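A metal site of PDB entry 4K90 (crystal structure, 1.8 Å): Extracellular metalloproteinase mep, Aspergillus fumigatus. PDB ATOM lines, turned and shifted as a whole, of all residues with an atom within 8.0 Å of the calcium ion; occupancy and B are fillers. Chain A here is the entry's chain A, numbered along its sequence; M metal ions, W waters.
The backbone NH of Gly 156 sits close to the side-chain carboxylate of Asp 133 (3.0 Å).
The side-chain amide nitrogen (ND2) of Asn 119 sits at hydrogen-bond distance from the backbone carbonyl oxygen (O) of Phe 113, at 3.2 Å.
O of Asp 133 is in hydrogen-bond range of N of Glu 121 (3.4 Å).
OD1 of Asp 155 lies close to NH1 of Arg 193, at 3.4 Å.
The backbone NH (N) of Asn 119 sits at hydrogen-bond distance from the backbone carbonyl oxygen (O) of Thr 114, 3.2 Å away.
The side-chain carboxylate (OE2) of Glu 121 lies within hydrogen-bond range of the side-chain amide nitrogen (ND2) of Asn 119 (2.9 Å).
OD2 of Asp 133 sits close to NH1 of Arg 193, at 3.0 Å.
The backbone NH (N) of Asp 155 sits at hydrogen-bond distance from the backbone carbonyl oxygen (O) of Pro 198 (3.0 Å).
The nearest printed residue that does not touch the calcium ion is Arg 193 (4.1 Å).
Water W2 bridges OD1 of Asn 119 (3.0 Å) and O of Glu 121 (3.1 Å).
Water W1 lies within hydrogen-bond range of O of Glu 115 (2.6 Å), OD2 of Asp 155 (2.7 Å) and N of Leu 130 (3.2 Å).
O of Leu 130 binds the calcium ion (2.3 Å).
O of Asn 119 is bound to the calcium ion, at 2.3 Å.
The side-chain carboxylate (OD1) of Asp 155 binds the calcium ion (2.4 Å).
The calcium ion is bound by water W2, at 2.4 Å.
Water W1 is bound to the calcium ion, 2.4 Å away.
The calcium ion is bound by OD2 of Asp 133 (2.5 Å).
The side-chain carboxylate (OD1) of Asp 133 is bound to the calcium ion (2.6 Å).
The calcium ion has seven donor atoms within binding distance.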
ATOM      1  N   PHE A 113     -15.900  -4.174   3.212  1.00  0.00           N
ATOM      2  CA  PHE A 113     -15.453  -2.779   3.153  1.00  0.00           C
ATOM      3  C   PHE A 113     -15.898  -2.068   4.422  1.00  0.00           C
ATOM      4  O   PHE A 113     -16.850  -1.254   4.413  1.00  0.00           O
ATOM      5  CB  PHE A 113     -15.968  -2.084   1.883  1.00  0.00           C
ATOM      6  CG  PHE A 113     -15.299  -0.749   1.585  1.00  0.00           C
ATOM      7  CD1 PHE A 113     -13.908  -0.579   1.741  1.00  0.00           C
ATOM      8  CD2 PHE A 113     -16.039   0.315   1.085  1.00  0.00           C
ATOM      9  CE1 PHE A 113     -13.294   0.668   1.434  1.00  0.00           C
ATOM     10  CE2 PHE A 113     -15.436   1.543   0.766  1.00  0.00           C
ATOM     11  CZ  PHE A 113     -14.051   1.714   0.935  1.00  0.00           C
ATOM     12  N   THR A 114     -15.179  -2.342   5.514  1.00  0.00           N
ATOM     13  CA  THR A 114     -15.505  -1.840   6.842  1.00  0.00           C
ATOM     14  C   THR A 114     -14.652  -0.631   7.188  1.00  0.00           C
ATOM     15  O   THR A 114     -13.904  -0.149   6.357  1.00  0.00           O
ATOM     16  CB  THR A 114     -15.282  -2.941   7.905  1.00  0.00           C
ATOM     17  OG1 THR A 114     -13.907  -3.346   7.846  1.00  0.00           O
ATOM     18  CG2 THR A 114     -16.175  -4.146   7.620  1.00  0.00           C
ATOM     19  N   GLU A 115     -14.751  -0.147   8.436  1.00  0.00           N
ATOM     20  CA  GLU A 115     -13.990   1.033   8.863  1.00  0.00           C
ATOM     21  C   GLU A 115     -12.472   0.800   8.704  1.00  0.00           C
ATOM     22  O   GLU A 115     -11.747   1.655   8.168  1.00  0.00           O
ATOM     23  CB  GLU A 115     -14.313   1.361  10.322  1.00  0.00           C
ATOM     24  CG  GLU A 115     -15.754   1.875  10.560  1.00  0.00           C
ATOM     25  CD  GLU A 115     -16.765   0.761  10.701  1.00  0.00           C
ATOM     26  OE1 GLU A 115     -16.385  -0.428  10.729  1.00  0.00           O
ATOM     27  OE2 GLU A 115     -17.982   1.075  10.781  1.00  0.00           O
ATOM     28  N   LYS A 116     -12.005  -0.356   9.171  1.00  0.00           N
ATOM     29  CA  LYS A 116     -10.553  -0.592   9.145  1.00  0.00           C
ATOM     30  C   LYS A 116     -10.047  -0.755   7.714  1.00  0.00           C
ATOM     31  O   LYS A 116      -8.858  -0.528   7.462  1.00  0.00           O
ATOM     32  CB  LYS A 116     -10.160  -1.782  10.015  1.00  0.00           C
ATOM     33  CG  LYS A 116     -10.816  -3.081   9.655  1.00  0.00           C
ATOM     34  CD  LYS A 116     -10.305  -4.168  10.602  1.00  0.00           C
ATOM     35  CE  LYS A 116     -11.021  -5.480  10.386  1.00  0.00           C
ATOM     36  NZ  LYS A 116     -10.539  -6.518  11.350  1.00  0.00           N
ATOM     37  N   ALA A 117     -10.941  -1.134   6.795  1.00  0.00           N
ATOM     38  CA  ALA A 117     -10.587  -1.268   5.363  1.00  0.00           C
ATOM     39  C   ALA A 117     -10.677   0.039   4.577  1.00  0.00           C
ATOM     40  O   ALA A 117     -10.564   0.038   3.349  1.00  0.00           O
ATOM     41  CB  ALA A 117     -11.452  -2.378   4.690  1.00  0.00           C
ATOM     42  N   GLY A 118     -10.859   1.164   5.274  1.00  0.00           N
ATOM     43  CA  GLY A 118     -10.830   2.485   4.654  1.00  0.00           C
ATOM     44  C   GLY A 118     -12.154   2.953   4.064  1.00  0.00           C
ATOM     45  O   GLY A 118     -12.172   3.692   3.073  1.00  0.00           O
ATOM     46  N   ASN A 119     -13.261   2.533   4.678  1.00  0.00           N
ATOM     47  CA  ASN A 119     -14.581   2.948   4.169  1.00  0.00           C
ATOM     48  C   ASN A 119     -14.940   4.419   4.434  1.00  0.00           C
ATOM     49  O   ASN A 119     -14.126   5.178   5.004  1.00  0.00           O
ATOM     50  CB  ASN A 119     -15.710   1.958   4.535  1.00  0.00           C
ATOM     51  CG  ASN A 119     -16.269   2.144   5.948  1.00  0.00           C
ATOM     52  OD1 ASN A 119     -15.828   2.980   6.724  1.00  0.00           O
ATOM     53  ND2 ASN A 119     -17.266   1.315   6.278  1.00  0.00           N
ATOM     54  N   PHE A 120     -16.132   4.811   4.001  1.00  0.00           N
ATOM     55  CA  PHE A 120     -16.567   6.204   4.044  1.00  0.00           C
ATOM     56  C   PHE A 120     -17.671   6.320   5.094  1.00  0.00           C
ATOM     57  O   PHE A 120     -18.783   5.894   4.848  1.00  0.00           O
ATOM     58  CB  PHE A 120     -17.145   6.615   2.688  1.00  0.00           C
ATOM     59  CG  PHE A 120     -16.138   6.600   1.590  1.00  0.00           C
ATOM     60  CD1 PHE A 120     -15.342   7.723   1.356  1.00  0.00           C
ATOM     61  CD2 PHE A 120     -15.997   5.489   0.772  1.00  0.00           C
ATOM     62  CE1 PHE A 120     -14.381   7.719   0.338  1.00  0.00           C
ATOM     63  CE2 PHE A 120     -15.055   5.462  -0.270  1.00  0.00           C
ATOM     64  CZ  PHE A 120     -14.245   6.601  -0.475  1.00  0.00           C
ATOM     65  N   GLU A 121     -17.307   6.801   6.279  1.00  0.00           N
ATOM     66  CA  GLU A 121     -18.214   6.947   7.437  1.00  0.00           C
ATOM     67  C   GLU A 121     -17.655   8.039   8.310  1.00  0.00           C
ATOM     68  O   GLU A 121     -16.462   8.061   8.603  1.00  0.00           O
ATOM     69  CB  GLU A 121     -18.262   5.681   8.297  1.00  0.00           C
ATOM     70  CG  GLU A 121     -18.935   4.500   7.661  1.00  0.00           C
ATOM     71  CD  GLU A 121     -18.945   3.300   8.577  1.00  0.00           C
ATOM     72  OE1 GLU A 121     -18.597   3.456   9.768  1.00  0.00           O
ATOM     73  OE2 GLU A 121     -19.301   2.195   8.112  1.00  0.00           O
ATOM     74  N   TYR A 122     -18.545   8.909   8.782  1.00  0.00           N
ATOM     75  CA  TYR A 122     -18.167  10.024   9.641  1.00  0.00           C
ATOM     76  C   TYR A 122     -17.647   9.566  11.018  1.00  0.00           C
ATOM     77  O   TYR A 122     -16.625  10.058  11.495  1.00  0.00           O
ATOM     78  CB  TYR A 122     -19.369  10.967   9.826  1.00  0.00           C
ATOM     79  CG  TYR A 122     -18.921  12.295  10.400  1.00  0.00           C
ATOM     80  CD1 TYR A 122     -18.434  13.293   9.562  1.00  0.00           C
ATOM     81  CD2 TYR A 122     -18.946  12.524  11.774  1.00  0.00           C
ATOM     82  CE1 TYR A 122     -17.995  14.500  10.057  1.00  0.00           C
ATOM     83  CE2 TYR A 122     -18.507  13.742  12.300  1.00  0.00           C
ATOM     84  CZ  TYR A 122     -18.033  14.717  11.426  1.00  0.00           C
ATOM     85  OH  TYR A 122     -17.591  15.933  11.898  1.00  0.00           O
ATOM     86  N   ASN A 123     -18.378   8.641  11.622  1.00  0.00           N
ATOM     87  CA  ASN A 123     -18.094   8.107  12.944  1.00  0.00           C
ATOM     88  C   ASN A 123     -17.781   6.620  12.815  1.00  0.00           C
ATOM     89  O   ASN A 123     -18.650   5.815  12.478  1.00  0.00           O
ATOM     90  CB  ASN A 123     -19.309   8.335  13.863  1.00  0.00           C
ATOM     91  CG  ASN A 123     -19.093   7.821  15.293  1.00  0.00           C
ATOM     92  OD1 ASN A 123     -18.059   7.228  15.625  1.00  0.00           O
ATOM     93  ND2 ASN A 123     -20.066   8.083  16.153  1.00  0.00           N
ATOM     94  N   THR A 124     -16.521   6.266  13.053  1.00  0.00           N
ATOM     95  CA  THR A 124     -16.093   4.872  12.881  1.00  0.00           C
ATOM     96  C   THR A 124     -16.535   3.978  14.050  1.00  0.00           C
ATOM     97  O   THR A 124     -16.324   2.761  14.032  1.00  0.00           O
ATOM     98  CB  THR A 124     -14.567   4.754  12.723  1.00  0.00           C
ATOM     99  OG1 THR A 124     -13.921   5.363  13.849  1.00  0.00           O
ATOM    100  CG2 THR A 124     -14.088   5.433  11.420  1.00  0.00           C
ATOM    101  N   GLY A 128     -11.949   1.140  14.049  1.00  0.00           N
ATOM    102  CA  GLY A 128     -10.707   1.264  13.285  1.00  0.00           C
ATOM    103  C   GLY A 128     -10.807   2.222  12.119  1.00  0.00           C
ATOM    104  O   GLY A 128     -11.864   2.832  11.894  1.00  0.00           O
ATOM    105  N   GLY A 129      -9.711   2.370  11.388  1.00  0.00           N
ATOM    106  CA  GLY A 129      -9.667   3.318  10.273  1.00  0.00           C
ATOM    107  C   GLY A 129      -9.730   4.773  10.724  1.00  0.00           C
ATOM    108  O   GLY A 129      -9.434   5.111  11.894  1.00  0.00           O
ATOM    109  N   LEU A 130     -10.077   5.652   9.787  1.00  0.00           N
ATOM    110  CA  LEU A 130     -10.196   7.084  10.079  1.00  0.00           C
ATOM    111  C   LEU A 130     -11.576   7.557   9.658  1.00  0.00           C
ATOM    112  O   LEU A 130     -12.022   7.248   8.557  1.00  0.00           O
ATOM    113  CB  LEU A 130      -9.104   7.889   9.364  1.00  0.00           C
ATOM    114  CG  LEU A 130      -7.657   7.617   9.813  1.00  0.00           C
ATOM    115  CD1 LEU A 130      -6.675   8.343   8.899  1.00  0.00           C
ATOM    116  CD2 LEU A 130      -7.424   7.987  11.281  1.00  0.00           C
ATOM    117  N   GLY A 131     -12.233   8.319  10.538  1.00  0.00           N
ATOM    118  CA  GLY A 131     -13.572   8.828  10.245  1.00  0.00           C
ATOM    119  C   GLY A 131     -13.575  10.184   9.570  1.00  0.00           C
ATOM    120  O   GLY A 131     -12.629  10.557   8.858  1.00  0.00           O
ATOM    121  N   ASN A 132     -14.651  10.939   9.809  1.00  0.00           N
ATOM    122  CA  ASN A 132     -14.859  12.236   9.195  1.00  0.00           C
ATOM    123  C   ASN A 132     -14.932  12.147   7.679  1.00  0.00           C
ATOM    124  O   ASN A 132     -14.701  13.134   6.987  1.00  0.00           O
ATOM    125  CB  ASN A 132     -13.774  13.242   9.629  1.00  0.00           C
ATOM    126  CG  ASN A 132     -13.929  13.677  11.086  1.00  0.00           C
ATOM    127  OD1 ASN A 132     -14.998  13.534  11.690  1.00  0.00           O
ATOM    128  ND2 ASN A 132     -12.853  14.181  11.674  1.00  0.00           N
ATOM    129  N   ASP A 133     -15.253  10.958   7.161  1.00  0.00           N
ATOM    130  CA  ASP A 133     -15.192  10.778   5.717  1.00  0.00           C
ATOM    131  C   ASP A 133     -16.383  10.078   5.087  1.00  0.00           C
ATOM    132  O   ASP A 133     -16.235   9.237   4.173  1.00  0.00           O
ATOM    133  CB  ASP A 133     -13.829  10.171   5.274  1.00  0.00           C
ATOM    134  CG  ASP A 133     -13.632   8.730   5.729  1.00  0.00           C
ATOM    135  OD1 ASP A 133     -14.442   8.178   6.531  1.00  0.00           O
ATOM    136  OD2 ASP A 133     -12.637   8.142   5.254  1.00  0.00           O
ATOM    137  N   TYR A 134     -17.588  10.466   5.523  1.00  0.00           N
ATOM    138  CA  TYR A 134     -18.769  10.150   4.742  1.00  0.00           C
ATOM    139  C   TYR A 134     -18.632  10.653   3.305  1.00  0.00           C
ATOM    140  O   TYR A 134     -17.723  11.419   3.005  1.00  0.00           O
ATOM    141  CB  TYR A 134     -20.068  10.718   5.364  1.00  0.00           C
ATOM    142  CG  TYR A 134     -20.114  12.195   5.768  1.00  0.00           C
ATOM    143  CD1 TYR A 134     -21.139  12.625   6.622  1.00  0.00           C
ATOM    144  CD2 TYR A 134     -19.212  13.149   5.281  1.00  0.00           C
ATOM    145  CE1 TYR A 134     -21.249  13.950   7.022  1.00  0.00           C
ATOM    146  CE2 TYR A 134     -19.318  14.504   5.666  1.00  0.00           C
ATOM    147  CZ  TYR A 134     -20.357  14.890   6.547  1.00  0.00           C
ATOM    148  OH  TYR A 134     -20.528  16.190   6.989  1.00  0.00           O
ATOM    149  N   PRO A 154      -7.255  10.121   0.481  1.00  0.00           N
ATOM    150  CA  PRO A 154      -6.981   9.007   1.380  1.00  0.00           C
ATOM    151  C   PRO A 154      -7.964   8.951   2.553  1.00  0.00           C
ATOM    152  O   PRO A 154      -8.707   9.904   2.788  1.00  0.00           O
ATOM    153  CB  PRO A 154      -5.558   9.283   1.893  1.00  0.00           C
ATOM    154  CG  PRO A 154      -4.974  10.231   0.867  1.00  0.00           C
ATOM    155  CD  PRO A 154      -6.136  11.081   0.455  1.00  0.00           C
ATOM    156  N   ASP A 155      -7.954   7.818   3.251  1.00  0.00           N
ATOM    157  CA  ASP A 155      -8.808   7.586   4.410  1.00  0.00           C
ATOM    158  C   ASP A 155      -8.758   8.762   5.371  1.00  0.00           C
ATOM    159  O   ASP A 155      -7.675   9.327   5.617  1.00  0.00           O
ATOM    160  CB  ASP A 155      -8.386   6.321   5.147  1.00  0.00           C
ATOM    161  CG  ASP A 155      -9.526   5.702   5.952  1.00  0.00           C
ATOM    162  OD1 ASP A 155     -10.712   6.081   5.718  1.00  0.00           O
ATOM    163  OD2 ASP A 155      -9.251   4.827   6.801  1.00  0.00           O
ATOM    164  N   GLY A 156      -9.921   9.163   5.873  1.00  0.00           N
ATOM    165  CA  GLY A 156      -9.996  10.298   6.808  1.00  0.00           C
ATOM    166  C   GLY A 156     -10.461  11.600   6.183  1.00  0.00           C
ATOM    167  O   GLY A 156     -10.667  12.581   6.918  1.00  0.00           O
ATOM    168  N   GLN A 157     -10.618  11.615   4.859  1.00  0.00           N
ATOM    169  CA  GLN A 157     -11.112  12.774   4.114  1.00  0.00           C
ATOM    170  C   GLN A 157     -12.308  12.365   3.281  1.00  0.00           C
ATOM    171  O   GLN A 157     -12.280  11.317   2.619  1.00  0.00           O
ATOM    172  CB  GLN A 157     -10.030  13.339   3.181  1.00  0.00           C
ATOM    173  CG  GLN A 157      -8.848  13.943   3.918  1.00  0.00           C
ATOM    174  CD  GLN A 157      -7.781  14.432   2.971  1.00  0.00           C
ATOM    175  OE1 GLN A 157      -7.973  15.401   2.246  1.00  0.00           O
ATOM    176  NE2 GLN A 157      -6.626  13.788   2.993  1.00  0.00           N
ATOM    177  N   PRO A 158     -13.379  13.177   3.279  1.00  0.00           N
ATOM    178  CA  PRO A 158     -14.592  12.737   2.587  1.00  0.00           C
ATOM    179  C   PRO A 158     -14.419  12.403   1.105  1.00  0.00           C
ATOM    180  O   PRO A 158     -13.632  13.045   0.407  1.00  0.00           O
ATOM    181  CB  PRO A 158     -15.550  13.937   2.748  1.00  0.00           C
ATOM    182  CG  PRO A 158     -15.031  14.688   3.937  1.00  0.00           C
ATOM    183  CD  PRO A 158     -13.548  14.501   3.925  1.00  0.00           C
ATOM    184  N   ARG A 193      -9.679   3.293  -2.358  1.00  0.00           N
ATOM    185  CA  ARG A 193      -9.380   3.059  -0.933  1.00  0.00           C
ATOM    186  C   ARG A 193      -8.724   1.706  -0.718  1.00  0.00           C
ATOM    187  O   ARG A 193      -7.661   1.627  -0.093  1.00  0.00           O
ATOM    188  CB  ARG A 193     -10.631   3.219  -0.054  1.00  0.00           C
ATOM    189  CG  ARG A 193     -11.089   4.680   0.102  1.00  0.00           C
ATOM    190  CD  ARG A 193     -10.159   5.482   1.006  1.00  0.00           C
ATOM    191  NE  ARG A 193     -10.473   6.914   1.105  1.00  0.00           N
ATOM    192  CZ  ARG A 193     -11.388   7.430   1.924  1.00  0.00           C
ATOM    193  NH1 ARG A 193     -12.141   6.605   2.681  1.00  0.00           N
ATOM    194  NH2 ARG A 193     -11.573   8.752   1.999  1.00  0.00           N
ATOM    195  N   PRO A 198      -5.807   1.880   2.683  1.00  0.00           N
ATOM    196  CA  PRO A 198      -6.574   3.110   2.894  1.00  0.00           C
ATOM    197  C   PRO A 198      -5.763   4.418   2.834  1.00  0.00           C
ATOM    198  O   PRO A 198      -6.312   5.438   2.386  1.00  0.00           O
ATOM    199  CB  PRO A 198      -7.181   2.892   4.285  1.00  0.00           C
ATOM    200  CG  PRO A 198      -7.407   1.358   4.325  1.00  0.00           C
ATOM    201  CD  PRO A 198      -6.099   0.855   3.698  1.00  0.00           C
HETATM  202 CA    CA M   1     -12.853   6.168   6.697  1.00  0.00          CA
HETATM  203  O   HOH W   1     -11.781   4.166   7.550  1.00  0.00           O
HETATM  204  O   HOH W   2     -14.773   5.492   8.006  1.00  0.00           O
